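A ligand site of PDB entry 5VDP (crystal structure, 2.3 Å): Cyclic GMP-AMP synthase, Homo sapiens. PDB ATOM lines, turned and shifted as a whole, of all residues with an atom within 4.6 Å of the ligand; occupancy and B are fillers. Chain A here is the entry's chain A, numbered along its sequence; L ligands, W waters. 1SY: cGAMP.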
ATOM      1  N   ASP A  68       9.622   2.438 -10.446  1.00  0.00           N
ATOM      2  CA  ASP A  68       9.518   3.351  -9.305  1.00  0.00           C
ATOM      3  C   ASP A  68       9.748   4.782  -9.742  1.00  0.00           C
ATOM      4  O   ASP A  68      10.873   5.180 -10.029  1.00  0.00           O
ATOM      5  CB  ASP A  68      10.507   2.952  -8.223  1.00  0.00           C
ATOM      6  CG  ASP A  68      10.573   3.967  -7.108  1.00  0.00           C
ATOM      7  OD1 ASP A  68      11.385   4.921  -7.206  1.00  0.00           O
ATOM      8  OD2 ASP A  68       9.817   3.813  -6.135  1.00  0.00           O
ATOM      9  N   TYR A  89      11.524  12.058   9.616  1.00  0.00           N
ATOM     10  CA  TYR A  89      10.178  12.567   9.419  1.00  0.00           C
ATOM     11  C   TYR A  89      10.015  14.012   9.900  1.00  0.00           C
ATOM     12  O   TYR A  89      10.584  14.431  10.911  1.00  0.00           O
ATOM     13  CB  TYR A  89       9.165  11.670  10.133  1.00  0.00           C
ATOM     14  CG  TYR A  89       9.235  10.242   9.661  1.00  0.00           C
ATOM     15  CD1 TYR A  89       8.507   9.820   8.562  1.00  0.00           C
ATOM     16  CD2 TYR A  89      10.038   9.306  10.313  1.00  0.00           C
ATOM     17  CE1 TYR A  89       8.563   8.522   8.122  1.00  0.00           C
ATOM     18  CE2 TYR A  89      10.102   8.003   9.885  1.00  0.00           C
ATOM     19  CZ  TYR A  89       9.357   7.613   8.799  1.00  0.00           C
ATOM     20  OH  TYR A  89       9.405   6.319   8.349  1.00  0.00           O
ATOM     21  N   GLY A 144       0.105  -0.684   3.136  1.00  0.00           N
ATOM     22  CA  GLY A 144       0.233  -0.159   4.482  1.00  0.00           C
ATOM     23  C   GLY A 144       1.486   0.651   4.735  1.00  0.00           C
ATOM     24  O   GLY A 144       2.603   0.128   4.652  1.00  0.00           O
ATOM     25  N   GLY A 145       1.300   1.931   5.069  1.00  0.00           N
ATOM     26  CA  GLY A 145       2.386   2.837   5.386  1.00  0.00           C
ATOM     27  C   GLY A 145       3.179   3.382   4.201  1.00  0.00           C
ATOM     28  O   GLY A 145       4.215   4.002   4.389  1.00  0.00           O
ATOM     29  N   SER A 146       2.695   3.149   2.983  1.00  0.00           N
ATOM     30  CA  SER A 146       3.439   3.574   1.796  1.00  0.00           C
ATOM     31  C   SER A 146       3.087   4.985   1.335  1.00  0.00           C
ATOM     32  O   SER A 146       1.926   5.398   1.361  1.00  0.00           O
ATOM     33  CB  SER A 146       3.213   2.598   0.645  1.00  0.00           C
ATOM     34  OG  SER A 146       3.936   3.037  -0.504  1.00  0.00           O
ATOM     35  N   PRO A 147       4.113   5.737   0.909  1.00  0.00           N
ATOM     36  CA  PRO A 147       3.904   7.081   0.358  1.00  0.00           C
ATOM     37  C   PRO A 147       3.528   7.015  -1.125  1.00  0.00           C
ATOM     38  O   PRO A 147       3.259   8.041  -1.747  1.00  0.00           O
ATOM     39  CB  PRO A 147       5.265   7.727   0.553  1.00  0.00           C
ATOM     40  CG  PRO A 147       6.230   6.570   0.380  1.00  0.00           C
ATOM     41  CD  PRO A 147       5.529   5.354   0.933  1.00  0.00           C
ATOM     42  N   ALA A 148       3.461   5.800  -1.672  1.00  0.00           N
ATOM     43  CA  ALA A 148       3.314   5.611  -3.103  1.00  0.00           C
ATOM     44  C   ALA A 148       1.891   5.240  -3.511  1.00  0.00           C
ATOM     45  O   ALA A 148       1.169   4.568  -2.761  1.00  0.00           O
ATOM     46  CB  ALA A 148       4.274   4.557  -3.596  1.00  0.00           C
ATOM     47  N   ASP A 160       5.257   2.348  -8.987  1.00  0.00           N
ATOM     48  CA  ASP A 160       5.100   3.134  -7.776  1.00  0.00           C
ATOM     49  C   ASP A 160       5.231   4.610  -8.107  1.00  0.00           C
ATOM     50  O   ASP A 160       6.292   5.063  -8.519  1.00  0.00           O
ATOM     51  CB  ASP A 160       6.137   2.742  -6.717  1.00  0.00           C
ATOM     52  CG  ASP A 160       5.678   1.593  -5.846  1.00  0.00           C
ATOM     53  OD1 ASP A 160       4.600   1.018  -6.114  1.00  0.00           O
ATOM     54  OD2 ASP A 160       6.397   1.243  -4.882  1.00  0.00           O
ATOM     55  N   THR A 162       5.275   8.222  -6.567  1.00  0.00           N
ATOM     56  CA  THR A 162       5.440   8.900  -5.297  1.00  0.00           C
ATOM     57  C   THR A 162       5.582  10.411  -5.442  1.00  0.00           C
ATOM     58  O   THR A 162       6.504  10.899  -6.104  1.00  0.00           O
ATOM     59  CB  THR A 162       6.666   8.359  -4.548  1.00  0.00           C
ATOM     60  OG1 THR A 162       6.465   6.959  -4.272  1.00  0.00           O
ATOM     61  CG2 THR A 162       6.886   9.095  -3.231  1.00  0.00           C
ATOM     62  N   VAL A 201       8.661  12.972   0.928  1.00  0.00           N
ATOM     63  CA  VAL A 201       7.563  12.141   0.431  1.00  0.00           C
ATOM     64  C   VAL A 201       6.547  11.941   1.543  1.00  0.00           C
ATOM     65  O   VAL A 201       6.906  11.987   2.714  1.00  0.00           O
ATOM     66  CB  VAL A 201       8.058  10.793  -0.120  1.00  0.00           C
ATOM     67  CG1 VAL A 201       9.029  11.009  -1.276  1.00  0.00           C
ATOM     68  CG2 VAL A 201       8.714   9.962   0.993  1.00  0.00           C
ATOM     69  N   LYS A 203       5.294   9.854   3.430  1.00  0.00           N
ATOM     70  CA  LYS A 203       5.348   8.666   4.277  1.00  0.00           C
ATOM     71  C   LYS A 203       5.362   9.138   5.719  1.00  0.00           C
ATOM     72  O   LYS A 203       6.258   9.868   6.121  1.00  0.00           O
ATOM     73  CB  LYS A 203       6.577   7.811   3.969  1.00  0.00           C
ATOM     74  CG  LYS A 203       7.054   6.952   5.144  1.00  0.00           C
ATOM     75  CD  LYS A 203       6.441   5.581   5.095  1.00  0.00           C
ATOM     76  CE  LYS A 203       6.481   4.881   6.449  1.00  0.00           C
ATOM     77  NZ  LYS A 203       5.276   5.229   7.279  1.00  0.00           N
ATOM     78  N   ARG A 217       8.551  12.484   4.964  1.00  0.00           N
ATOM     79  CA  ARG A 217       9.856  11.875   5.215  1.00  0.00           C
ATOM     80  C   ARG A 217      10.868  12.279   4.139  1.00  0.00           C
ATOM     81  O   ARG A 217      10.506  12.497   2.982  1.00  0.00           O
ATOM     82  CB  ARG A 217       9.747  10.358   5.289  1.00  0.00           C
ATOM     83  CG  ARG A 217      10.956   9.720   5.968  1.00  0.00           C
ATOM     84  CD  ARG A 217      11.832   8.996   4.962  1.00  0.00           C
ATOM     85  NE  ARG A 217      11.146   7.836   4.447  1.00  0.00           N
ATOM     86  CZ  ARG A 217      11.115   7.487   3.173  1.00  0.00           C
ATOM     87  NH1 ARG A 217      11.750   8.213   2.269  1.00  0.00           N
ATOM     88  NH2 ARG A 217      10.443   6.404   2.804  1.00  0.00           N
ATOM     89  N   LEU A 218      12.121  12.434   4.549  1.00  0.00           N
ATOM     90  CA  LEU A 218      13.209  12.721   3.610  1.00  0.00           C
ATOM     91  C   LEU A 218      13.438  11.592   2.596  1.00  0.00           C
ATOM     92  O   LEU A 218      13.309  10.399   2.926  1.00  0.00           O
ATOM     93  CB  LEU A 218      14.526  12.958   4.368  1.00  0.00           C
ATOM     94  CG  LEU A 218      14.591  14.180   5.273  1.00  0.00           C
ATOM     95  CD1 LEU A 218      15.857  14.169   6.108  1.00  0.00           C
ATOM     96  CD2 LEU A 218      14.490  15.452   4.428  1.00  0.00           C
ATOM     97  N   SER A 219      13.785  11.979   1.375  1.00  0.00           N
ATOM     98  CA  SER A 219      14.164  11.037   0.336  1.00  0.00           C
ATOM     99  C   SER A 219      15.338  11.613  -0.443  1.00  0.00           C
ATOM    100  O   SER A 219      15.383  12.811  -0.721  1.00  0.00           O
ATOM    101  CB  SER A 219      12.979  10.754  -0.579  1.00  0.00           C
ATOM    102  OG  SER A 219      13.315   9.908  -1.658  1.00  0.00           O
ATOM    103  N   SER A 221      16.636   9.779  -3.363  1.00  0.00           N
ATOM    104  CA  SER A 221      16.754   8.804  -4.429  1.00  0.00           C
ATOM    105  C   SER A 221      17.583   9.355  -5.564  1.00  0.00           C
ATOM    106  O   SER A 221      18.266   8.608  -6.253  1.00  0.00           O
ATOM    107  CB  SER A 221      15.388   8.369  -4.948  1.00  0.00           C
ATOM    108  OG  SER A 221      14.661   7.695  -3.941  1.00  0.00           O
ATOM    109  N   LYS A 273       9.030  -7.474   5.047  1.00  0.00           N
ATOM    110  CA  LYS A 273       9.477  -6.124   5.351  1.00  0.00           C
ATOM    111  C   LYS A 273      10.844  -5.802   4.737  1.00  0.00           C
ATOM    112  O   LYS A 273      11.242  -4.651   4.717  1.00  0.00           O
ATOM    113  CB  LYS A 273       9.525  -5.910   6.860  1.00  0.00           C
ATOM    114  CG  LYS A 273       8.156  -6.065   7.540  1.00  0.00           C
ATOM    115  CD  LYS A 273       7.952  -5.048   8.629  1.00  0.00           C
ATOM    116  CE  LYS A 273       6.649  -5.301   9.370  1.00  0.00           C
ATOM    117  NZ  LYS A 273       5.487  -5.316   8.415  1.00  0.00           N
ATOM    118  N   SER A 275      13.610  -5.235   1.741  1.00  0.00           N
ATOM    119  CA  SER A 275      13.480  -4.782   0.383  1.00  0.00           C
ATOM    120  C   SER A 275      14.818  -4.430  -0.217  1.00  0.00           C
ATOM    121  O   SER A 275      15.830  -4.326   0.506  1.00  0.00           O
ATOM    122  CB  SER A 275      12.524  -3.577   0.279  1.00  0.00           C
ATOM    123  OG  SER A 275      13.149  -2.342   0.594  1.00  0.00           O
ATOM    124  N   TYR A 277      15.859  -1.768  -1.008  1.00  0.00           N
ATOM    125  CA  TYR A 277      16.384  -0.556  -0.367  1.00  0.00           C
ATOM    126  C   TYR A 277      17.336  -0.907   0.777  1.00  0.00           C
ATOM    127  O   TYR A 277      18.290  -0.163   1.061  1.00  0.00           O
ATOM    128  CB  TYR A 277      15.257   0.371   0.168  1.00  0.00           C
ATOM    129  CG  TYR A 277      15.829   1.702   0.577  1.00  0.00           C
ATOM    130  CD1 TYR A 277      16.090   2.678  -0.385  1.00  0.00           C
ATOM    131  CD2 TYR A 277      16.172   1.977   1.901  1.00  0.00           C
ATOM    132  CE1 TYR A 277      16.660   3.898  -0.054  1.00  0.00           C
ATOM    133  CE2 TYR A 277      16.741   3.201   2.251  1.00  0.00           C
ATOM    134  CZ  TYR A 277      16.981   4.160   1.254  1.00  0.00           C
ATOM    135  OH  TYR A 277      17.549   5.384   1.542  1.00  0.00           O
ATOM    136  N   HIS A 278      17.080  -2.028   1.442  1.00  0.00           N
ATOM    137  CA  HIS A 278      17.951  -2.471   2.526  1.00  0.00           C
ATOM    138  C   HIS A 278      19.285  -2.913   1.949  1.00  0.00           C
ATOM    139  O   HIS A 278      20.371  -2.619   2.485  1.00  0.00           O
ATOM    140  CB  HIS A 278      17.305  -3.606   3.326  1.00  0.00           C
ATOM    141  CG  HIS A 278      16.077  -3.178   4.067  1.00  0.00           C
ATOM    142  ND1 HIS A 278      14.866  -3.822   3.930  1.00  0.00           N
ATOM    143  CD2 HIS A 278      15.863  -2.154   4.930  1.00  0.00           C
ATOM    144  CE1 HIS A 278      13.961  -3.228   4.688  1.00  0.00           C
ATOM    145  NE2 HIS A 278      14.540  -2.207   5.299  1.00  0.00           N
ATOM    146  N   ASN A 323      20.475   4.296   7.776  1.00  0.00           N
ATOM    147  CA  ASN A 323      20.169   5.021   6.566  1.00  0.00           C
ATOM    148  C   ASN A 323      21.455   5.679   6.084  1.00  0.00           C
ATOM    149  O   ASN A 323      22.152   6.298   6.873  1.00  0.00           O
ATOM    150  CB  ASN A 323      19.101   6.086   6.813  1.00  0.00           C
ATOM    151  CG  ASN A 323      18.756   6.853   5.574  1.00  0.00           C
ATOM    152  OD1 ASN A 323      19.595   7.599   5.051  1.00  0.00           O
ATOM    153  ND2 ASN A 323      17.538   6.658   5.071  1.00  0.00           N
ATOM    154  N   PHE A 329      19.013   7.004  11.847  1.00  0.00           N
ATOM    155  CA  PHE A 329      17.829   6.253  11.477  1.00  0.00           C
ATOM    156  C   PHE A 329      18.186   4.775  11.174  1.00  0.00           C
ATOM    157  O   PHE A 329      18.836   4.471  10.172  1.00  0.00           O
ATOM    158  CB  PHE A 329      17.119   6.878  10.278  1.00  0.00           C
ATOM    159  CG  PHE A 329      15.781   6.276  10.011  1.00  0.00           C
ATOM    160  CD1 PHE A 329      14.690   6.593  10.794  1.00  0.00           C
ATOM    161  CD2 PHE A 329      15.605   5.367   8.977  1.00  0.00           C
ATOM    162  CE1 PHE A 329      13.456   6.028  10.558  1.00  0.00           C
ATOM    163  CE2 PHE A 329      14.357   4.796   8.722  1.00  0.00           C
ATOM    164  CZ  PHE A 329      13.286   5.126   9.523  1.00  0.00           C
ATOM    165  N   LEU A 331      17.274   1.303  10.000  1.00  0.00           N
ATOM    166  CA  LEU A 331      16.314   0.570   9.180  1.00  0.00           C
ATOM    167  C   LEU A 331      16.066  -0.829   9.733  1.00  0.00           C
ATOM    168  O   LEU A 331      15.060  -1.456   9.403  1.00  0.00           O
ATOM    169  CB  LEU A 331      16.790   0.503   7.730  1.00  0.00           C
ATOM    170  CG  LEU A 331      17.014   1.816   6.961  1.00  0.00           C
ATOM    171  CD1 LEU A 331      17.841   1.592   5.701  1.00  0.00           C
ATOM    172  CD2 LEU A 331      15.671   2.402   6.583  1.00  0.00           C
HETATM  173  C2  1SY L   1      14.176   5.959   2.257  1.00  0.00           C
HETATM  174  N01 1SY L   1      13.208   5.673  -1.234  1.00  0.00           N
HETATM  175  C6  1SY L   1      13.409   5.343   0.157  1.00  0.00           C
HETATM  176  N1  1SY L   1      13.975   6.233   0.971  1.00  0.00           N
HETATM  177  N3  1SY L   1      13.803   4.814   2.787  1.00  0.00           N
HETATM  178  C4  1SY L   1      13.221   3.869   2.027  1.00  0.00           C
HETATM  179  C5  1SY L   1      13.000   4.108   0.687  1.00  0.00           C
HETATM  180  N7  1SY L   1      12.409   3.002   0.188  1.00  0.00           N
HETATM  181  C8  1SY L   1      12.271   2.110   1.159  1.00  0.00           C
HETATM  182  N9  1SY L   1      12.753   2.620   2.284  1.00  0.00           N
HETATM  183  C1' 1SY L   1      12.787   1.936   3.512  1.00  0.00           C
HETATM  184  C2' 1SY L   1      11.651   2.259   4.439  1.00  0.00           C
HETATM  185  O2' 1SY L   1      12.117   2.404   5.790  1.00  0.00           O
HETATM  186  C3' 1SY L   1      10.751   1.105   4.285  1.00  0.00           C
HETATM  187  C4' 1SY L   1      11.639  -0.037   4.008  1.00  0.00           C
HETATM  188  C16 1SY L   1      10.887  -1.106   3.238  1.00  0.00           C
HETATM  189  O17 1SY L   1      10.799  -0.612   1.921  1.00  0.00           O
HETATM  190  P18 1SY L   1       9.693  -1.296   0.878  1.00  0.00           P
HETATM  191  O19 1SY L   1      10.305  -1.734  -0.421  1.00  0.00           O
HETATM  192  O20 1SY L   1       8.347  -0.302   0.604  1.00  0.00           O
HETATM  193  C21 1SY L   1       7.730   0.421   1.717  1.00  0.00           C
HETATM  194  C22 1SY L   1       6.675  -0.331   2.318  1.00  0.00           C
HETATM  195  O23 1SY L   1       5.954  -1.040   1.293  1.00  0.00           O
HETATM  196  C24 1SY L   1       5.775   0.739   2.930  1.00  0.00           C
HETATM  197  C25 1SY L   1       6.130   1.072   4.313  1.00  0.00           C
HETATM  198  O26 1SY L   1       7.508   0.700   4.468  1.00  0.00           O
HETATM  199  P27 1SY L   1       8.535   1.510   5.515  1.00  0.00           P
HETATM  200  O28 1SY L   1      10.003   0.848   5.476  1.00  0.00           O
HETATM  201  O29 1SY L   1       8.601   3.008   5.374  1.00  0.00           O
HETATM  202  O30 1SY L   1       7.986   1.277   6.911  1.00  0.00           O
HETATM  203  O31 1SY L   1       6.029   1.924   2.127  1.00  0.00           O
HETATM  204  C32 1SY L   1       7.017   1.559   1.162  1.00  0.00           C
HETATM  205  N33 1SY L   1       7.872   2.689   0.993  1.00  0.00           N
HETATM  206  C34 1SY L   1       8.465   3.377   1.965  1.00  0.00           C
HETATM  207  N35 1SY L   1       9.173   4.369   1.420  1.00  0.00           N
HETATM  208  C36 1SY L   1       8.189   3.237  -0.181  1.00  0.00           C
HETATM  209  C37 1SY L   1       9.014   4.311   0.094  1.00  0.00           C
HETATM  210  C38 1SY L   1       9.562   5.156  -1.028  1.00  0.00           C
HETATM  211  N39 1SY L   1       9.207   4.830  -2.383  1.00  0.00           N
HETATM  212  C40 1SY L   1       8.330   3.700  -2.634  1.00  0.00           C
HETATM  213  N41 1SY L   1       7.963   3.339  -4.011  1.00  0.00           N
HETATM  214  N42 1SY L   1       7.815   2.885  -1.549  1.00  0.00           N
HETATM  215  O43 1SY L   1      10.276   6.080  -0.768  1.00  0.00           O
HETATM  216  O44 1SY L   1       9.154  -2.532   1.545  1.00  0.00           O
HETATM  217  O4' 1SY L   1      12.642   0.513   3.167  1.00  0.00           O
HETATM  218  O   HOH W   1      10.186   4.983   6.149  1.00  0.00           O
HETATM  219  O   HOH W   2      16.389   8.171   0.875  1.00  0.00           O
HETATM  220  O   HOH W   3      10.614   1.095  -2.708  1.00  0.00           O
HETATM  221  O   HOH W   4      14.814   5.230   5.572  1.00  0.00           O
HETATM  222  O   HOH W   5      10.067   6.229  -4.620  1.00  0.00           O
HETATM  223  O   HOH W   6       7.922   5.747  -6.176  1.00  0.00           O
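The side-chain hydroxyl of Ser 275 lies close to an oxygen (O19) of the ligand (3.1 Å). The side-chain carboxylate of Asp 160 sits at hydrogen-bond distance from a nitrogen (N41) of the ligand (2.8 Å). N35 of the ligand sits at hydrogen-bond distance from NH2 of Arg 217. The side-chain carboxylate (OD2) of Asp 68 sits at hydrogen-bond distance from a nitrogen (N41) of the ligand, at 2.9 Å.
A ring nitrogen (ND1) of His 278 sits at hydrogen-bond distance from the backbone NH (N) of Ser 275. O of Gly 145 lies close to NZ of Lys 203. The side-chain hydroxyl of Ser 275 sits close to the backbone NH of Tyr 277 (3.2 Å). OG of Ser 221 lies within hydrogen-bond range of OG of Ser 219, at 3.5 Å. OG of Ser 146 is in hydrogen-bond range of N of Ala 148, 3.0 Å away. The backbone carbonyl oxygen (O) of Arg 217 is in hydrogen-bond range of the backbone NH (N) of Val 201 (2.8 Å).
Residues that only touch the ligand: Lys 203 (3.0 Å), Ser 146 (3.1 Å), Tyr 277 (3.4 Å), Gly 145 (3.5 Å), Pro 147 (3.5 Å), Leu 331 (3.6 Å), Gly 144 (3.7 Å), Ser 221 (3.7 Å), His 278 (3.8 Å), Lys 273 (3.9 Å), Ala 148 (3.9 Å) and Thr 162 (3.9 Å). Hydrophobic or aromatic side chains that line the ligand: Pro 147, Ala 148, Tyr 277 and Leu 331. 16 residues have an atom within 4 Å of the ligand: Asp 68, Gly 144, Gly 145, Ser 146, Pro 147, Ala 148, Asp 160, Thr 162, Lys 203, Arg 217, Ser 221, Lys 273, Ser 275, Tyr 277, His 278 and Leu 331.
Water W1 lies within hydrogen-bond range of O29 of the ligand (2.6 Å), OH of Tyr 89 (2.7 Å) and NE of Arg 217 (3.5 Å). Water W5 bridges a nitrogen (N39) of the ligand and the side-chain carboxylate (OD2) of Asp 68. Water W4 bridges N3 of the ligand (3.0 Å) and ND2 of Asn 323 (3.1 Å). Water W2 bridges OH of Tyr 277 (3.1 Å) and N1 of the ligand (3.1 Å). Water W6 lies within hydrogen-bond range of the side-chain hydroxyl (OG1) of Thr 162, the side-chain carboxylate (OD2) of Asp 68, the backbone carbonyl oxygen (O) of Asp 160 and a nitrogen (N41) of the ligand.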
